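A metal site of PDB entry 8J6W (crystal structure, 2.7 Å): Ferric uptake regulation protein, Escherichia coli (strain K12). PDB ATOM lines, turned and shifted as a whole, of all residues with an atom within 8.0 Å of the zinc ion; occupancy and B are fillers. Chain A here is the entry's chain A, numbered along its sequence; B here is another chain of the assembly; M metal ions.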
ATOM      1  N   HIS A  87       3.114 -16.683 -26.647  1.00  0.00           N
ATOM      2  CA  HIS A  87       3.316 -15.491 -27.468  1.00  0.00           C
ATOM      3  C   HIS A  87       4.554 -14.727 -27.022  1.00  0.00           C
ATOM      4  O   HIS A  87       4.742 -14.437 -25.839  1.00  0.00           O
ATOM      5  CB  HIS A  87       2.134 -14.535 -27.407  1.00  0.00           C
ATOM      6  CG  HIS A  87       2.326 -13.319 -28.247  1.00  0.00           C
ATOM      7  ND1 HIS A  87       2.268 -13.352 -29.625  1.00  0.00           N
ATOM      8  CD2 HIS A  87       2.626 -12.037 -27.918  1.00  0.00           C
ATOM      9  CE1 HIS A  87       2.491 -12.139 -30.100  1.00  0.00           C
ATOM     10  NE2 HIS A  87       2.705 -11.325 -29.085  1.00  0.00           N
ATOM     11  N   HIS A  88       5.375 -14.371 -27.996  1.00  0.00           N
ATOM     12  CA  HIS A  88       6.481 -13.463 -27.739  1.00  0.00           C
ATOM     13  C   HIS A  88       6.635 -12.582 -28.972  1.00  0.00           C
ATOM     14  O   HIS A  88       6.027 -12.822 -30.006  1.00  0.00           O
ATOM     15  CB  HIS A  88       7.760 -14.237 -27.432  1.00  0.00           C
ATOM     16  CG  HIS A  88       8.156 -15.190 -28.509  1.00  0.00           C
ATOM     17  ND1 HIS A  88       8.107 -16.555 -28.346  1.00  0.00           N
ATOM     18  CD2 HIS A  88       8.576 -14.978 -29.778  1.00  0.00           C
ATOM     19  CE1 HIS A  88       8.517 -17.141 -29.458  1.00  0.00           C
ATOM     20  NE2 HIS A  88       8.802 -16.208 -30.337  1.00  0.00           N
ATOM     21  N   ASP A  89       7.457 -11.558 -28.836  1.00  0.00           N
ATOM     22  CA  ASP A  89       7.849 -10.727 -29.957  1.00  0.00           C
ATOM     23  C   ASP A  89       9.352 -10.911 -30.138  1.00  0.00           C
ATOM     24  O   ASP A  89       9.957 -11.792 -29.521  1.00  0.00           O
ATOM     25  CB  ASP A  89       7.399  -9.291 -29.725  1.00  0.00           C
ATOM     26  CG  ASP A  89       5.892  -9.135 -29.832  1.00  0.00           C
ATOM     27  OD1 ASP A  89       5.308  -9.451 -30.902  1.00  0.00           O
ATOM     28  OD2 ASP A  89       5.297  -8.755 -28.812  1.00  0.00           O
ATOM     29  N   HIS A  90       9.962 -10.105 -30.993  1.00  0.00           N
ATOM     30  CA  HIS A  90      11.319 -10.413 -31.434  1.00  0.00           C
ATOM     31  C   HIS A  90      12.233  -9.209 -31.342  1.00  0.00           C
ATOM     32  O   HIS A  90      11.912  -8.145 -31.881  1.00  0.00           O
ATOM     33  CB  HIS A  90      11.318 -10.965 -32.855  1.00  0.00           C
ATOM     34  CG  HIS A  90      10.453 -12.168 -33.016  1.00  0.00           C
ATOM     35  ND1 HIS A  90       9.164 -12.103 -33.489  1.00  0.00           N
ATOM     36  CD2 HIS A  90      10.697 -13.479 -32.772  1.00  0.00           C
ATOM     37  CE1 HIS A  90       8.650 -13.314 -33.528  1.00  0.00           C
ATOM     38  NE2 HIS A  90       9.558 -14.166 -33.116  1.00  0.00           N
ATOM     39  N   PHE A 102      10.842 -12.102 -26.360  1.00  0.00           N
ATOM     40  CA  PHE A 102      10.457 -11.277 -25.226  1.00  0.00           C
ATOM     41  C   PHE A 102       8.949 -11.084 -25.240  1.00  0.00           C
ATOM     42  O   PHE A 102       8.306 -11.089 -26.298  1.00  0.00           O
ATOM     43  CB  PHE A 102      11.167  -9.904 -25.207  1.00  0.00           C
ATOM     44  CG  PHE A 102      10.647  -8.887 -26.227  1.00  0.00           C
ATOM     45  CD1 PHE A 102       9.570  -8.058 -25.949  1.00  0.00           C
ATOM     46  CD2 PHE A 102      11.307  -8.712 -27.435  1.00  0.00           C
ATOM     47  CE1 PHE A 102       9.103  -7.138 -26.879  1.00  0.00           C
ATOM     48  CE2 PHE A 102      10.861  -7.782 -28.373  1.00  0.00           C
ATOM     49  CZ  PHE A 102       9.755  -6.999 -28.090  1.00  0.00           C
ATOM     50  N   SER A 103       8.391 -10.912 -24.045  1.00  0.00           N
ATOM     51  CA  SER A 103       6.985 -10.611 -23.907  1.00  0.00           C
ATOM     52  C   SER A 103       6.835  -9.611 -22.777  1.00  0.00           C
ATOM     53  O   SER A 103       7.450  -9.769 -21.709  1.00  0.00           O
ATOM     54  CB  SER A 103       6.140 -11.870 -23.640  1.00  0.00           C
ATOM     55  OG  SER A 103       4.782 -11.512 -23.431  1.00  0.00           O
ATOM     56  N   ASP A 104       6.049  -8.567 -23.026  1.00  0.00           N
ATOM     57  CA  ASP A 104       5.808  -7.482 -22.088  1.00  0.00           C
ATOM     58  C   ASP A 104       4.296  -7.415 -21.896  1.00  0.00           C
ATOM     59  O   ASP A 104       3.558  -7.262 -22.875  1.00  0.00           O
ATOM     60  CB  ASP A 104       6.386  -6.165 -22.627  1.00  0.00           C
ATOM     61  CG  ASP A 104       6.583  -5.100 -21.547  1.00  0.00           C
ATOM     62  OD1 ASP A 104       5.573  -4.704 -20.906  1.00  0.00           O
ATOM     63  OD2 ASP A 104       7.736  -4.637 -21.362  1.00  0.00           O
ATOM     64  N   ILE A 107       2.829  -3.881 -22.617  1.00  0.00           N
ATOM     65  CA  ILE A 107       2.711  -3.536 -24.032  1.00  0.00           C
ATOM     66  C   ILE A 107       1.528  -4.267 -24.665  1.00  0.00           C
ATOM     67  O   ILE A 107       0.685  -3.646 -25.301  1.00  0.00           O
ATOM     68  CB  ILE A 107       4.017  -3.843 -24.779  1.00  0.00           C
ATOM     69  CG1 ILE A 107       5.153  -2.952 -24.275  1.00  0.00           C
ATOM     70  CG2 ILE A 107       3.829  -3.619 -26.282  1.00  0.00           C
ATOM     71  CD1 ILE A 107       6.421  -3.041 -25.117  1.00  0.00           C
ATOM     72  N   GLU A 108       1.447  -5.587 -24.485  1.00  0.00           N
ATOM     73  CA  GLU A 108       0.334  -6.337 -25.054  1.00  0.00           C
ATOM     74  C   GLU A 108      -1.003  -5.765 -24.585  1.00  0.00           C
ATOM     75  O   GLU A 108      -2.011  -5.889 -25.285  1.00  0.00           O
ATOM     76  CB  GLU A 108       0.399  -7.835 -24.693  1.00  0.00           C
ATOM     77  CG  GLU A 108       1.739  -8.520 -24.981  1.00  0.00           C
ATOM     78  CD  GLU A 108       2.047  -8.749 -26.472  1.00  0.00           C
ATOM     79  OE1 GLU A 108       1.141  -9.109 -27.258  1.00  0.00           O
ATOM     80  OE2 GLU A 108       3.219  -8.598 -26.862  1.00  0.00           O
ATOM     81  N   GLN A 111      -1.511  -2.269 -26.425  1.00  0.00           N
ATOM     82  CA  GLN A 111      -1.850  -2.575 -27.810  1.00  0.00           C
ATOM     83  C   GLN A 111      -3.337  -2.860 -27.941  1.00  0.00           C
ATOM     84  O   GLN A 111      -3.999  -2.370 -28.865  1.00  0.00           O
ATOM     85  CB  GLN A 111      -1.028  -3.744 -28.301  1.00  0.00           C
ATOM     86  CG  GLN A 111       0.412  -3.404 -28.618  1.00  0.00           C
ATOM     87  CD  GLN A 111       1.241  -4.627 -29.004  1.00  0.00           C
ATOM     88  OE1 GLN A 111       0.762  -5.761 -28.945  1.00  0.00           O
ATOM     89  NE2 GLN A 111       2.491  -4.401 -29.371  1.00  0.00           N
ATOM     90  N   LEU A 122      -8.279  -5.918 -31.274  1.00  0.00           N
ATOM     91  CA  LEU A 122      -6.993  -6.438 -31.701  1.00  0.00           C
ATOM     92  C   LEU A 122      -7.022  -7.938 -31.859  1.00  0.00           C
ATOM     93  O   LEU A 122      -7.303  -8.662 -30.895  1.00  0.00           O
ATOM     94  CB  LEU A 122      -5.919  -6.055 -30.674  1.00  0.00           C
ATOM     95  CG  LEU A 122      -4.497  -6.359 -31.129  1.00  0.00           C
ATOM     96  CD1 LEU A 122      -4.073  -5.379 -32.270  1.00  0.00           C
ATOM     97  CD2 LEU A 122      -3.613  -6.202 -29.943  1.00  0.00           C
ATOM     98  N   ASN A 124      -4.366  -9.591 -34.212  1.00  0.00           N
ATOM     99  CA  ASN A 124      -3.003 -10.034 -34.449  1.00  0.00           C
ATOM    100  C   ASN A 124      -2.088  -8.816 -34.461  1.00  0.00           C
ATOM    101  O   ASN A 124      -2.551  -7.673 -34.580  1.00  0.00           O
ATOM    102  CB  ASN A 124      -2.905 -10.821 -35.759  1.00  0.00           C
ATOM    103  CG  ASN A 124      -1.560 -11.506 -35.939  1.00  0.00           C
ATOM    104  OD1 ASN A 124      -0.893 -11.857 -34.967  1.00  0.00           O
ATOM    105  ND2 ASN A 124      -1.170 -11.723 -37.184  1.00  0.00           N
ATOM    106  N   HIS A 125      -0.795  -9.078 -34.319  1.00  0.00           N
ATOM    107  CA  HIS A 125       0.187  -8.009 -34.295  1.00  0.00           C
ATOM    108  C   HIS A 125       1.560  -8.608 -34.488  1.00  0.00           C
ATOM    109  O   HIS A 125       1.788  -9.781 -34.190  1.00  0.00           O
ATOM    110  CB  HIS A 125       0.123  -7.209 -32.992  1.00  0.00           C
ATOM    111  CG  HIS A 125       0.542  -7.972 -31.785  1.00  0.00           C
ATOM    112  ND1 HIS A 125      -0.300  -8.832 -31.116  1.00  0.00           N
ATOM    113  CD2 HIS A 125       1.720  -8.007 -31.113  1.00  0.00           C
ATOM    114  CE1 HIS A 125       0.340  -9.373 -30.092  1.00  0.00           C
ATOM    115  NE2 HIS A 125       1.562  -8.889 -30.071  1.00  0.00           N
ATOM    116  N   SER A 126       2.475  -7.793 -34.998  1.00  0.00           N
ATOM    117  CA  SER A 126       3.875  -8.174 -35.062  1.00  0.00           C
ATOM    118  C   SER A 126       4.719  -7.003 -34.618  1.00  0.00           C
ATOM    119  O   SER A 126       4.500  -5.854 -35.034  1.00  0.00           O
ATOM    120  CB  SER A 126       4.279  -8.665 -36.454  1.00  0.00           C
ATOM    121  OG  SER A 126       4.422  -7.613 -37.363  1.00  0.00           O
ATOM    122  N   LEU A 127       5.681  -7.297 -33.748  1.00  0.00           N
ATOM    123  CA  LEU A 127       6.535  -6.280 -33.176  1.00  0.00           C
ATOM    124  C   LEU A 127       7.962  -6.756 -33.352  1.00  0.00           C
ATOM    125  O   LEU A 127       8.362  -7.735 -32.740  1.00  0.00           O
ATOM    126  CB  LEU A 127       6.190  -6.032 -31.706  1.00  0.00           C
ATOM    127  CG  LEU A 127       7.137  -5.195 -30.854  1.00  0.00           C
ATOM    128  CD1 LEU A 127       7.491  -3.865 -31.496  1.00  0.00           C
ATOM    129  CD2 LEU A 127       6.438  -4.984 -29.536  1.00  0.00           C
ATOM    130  N   LEU B 127       6.092  -1.862 -35.698  1.00  0.00           N
ATOM    131  CA  LEU B 127       5.010  -2.362 -34.881  1.00  0.00           C
ATOM    132  C   LEU B 127       3.748  -2.262 -35.714  1.00  0.00           C
ATOM    133  O   LEU B 127       3.296  -1.166 -36.012  1.00  0.00           O
ATOM    134  CB  LEU B 127       4.898  -1.579 -33.573  1.00  0.00           C
ATOM    135  CG  LEU B 127       3.666  -1.774 -32.695  1.00  0.00           C
ATOM    136  CD1 LEU B 127       3.370  -3.235 -32.407  1.00  0.00           C
ATOM    137  CD2 LEU B 127       3.939  -1.021 -31.419  1.00  0.00           C
ATOM    138  N   LEU B 129      -0.247  -3.367 -35.899  1.00  0.00           N
ATOM    139  CA  LEU B 129      -1.403  -3.880 -35.196  1.00  0.00           C
ATOM    140  C   LEU B 129      -2.490  -4.202 -36.202  1.00  0.00           C
ATOM    141  O   LEU B 129      -2.740  -3.434 -37.131  1.00  0.00           O
ATOM    142  CB  LEU B 129      -1.935  -2.876 -34.161  1.00  0.00           C
ATOM    143  CG  LEU B 129      -1.011  -2.495 -32.998  1.00  0.00           C
ATOM    144  CD1 LEU B 129      -1.719  -1.616 -31.991  1.00  0.00           C
ATOM    145  CD2 LEU B 129      -0.430  -3.739 -32.326  1.00  0.00           C
HETATM  146 ZN    ZN M   1       3.398  -9.177 -28.830  1.00  0.00          ZN
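The zinc ion is bound by OD2 of Asp 89, OE2 of Glu 108, NE2 of His 125 and NE2 of His 87.
The zinc ion has four donor atoms within binding distance.
Slightly farther from the zinc ion lies the side-chain carboxylate (OE1) of Glu 108 (2.8 Å).
Slightly farther from the zinc ion lies OD1 of Asp 89 (2.8 Å).
Within 4 Å of the zinc ion: His 87, Asp 89, Glu 108 and His 125.
Along chain A the residues within 4 Å of the zinc ion span positions 87 to 125.
A ring nitrogen (NE2) of His 125 sits close to the side-chain amide oxygen (OE1) of Gln 111 (3.4 Å).
N of Asp 89 lies within hydrogen-bond range of O of Phe 102, at 2.7 Å.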
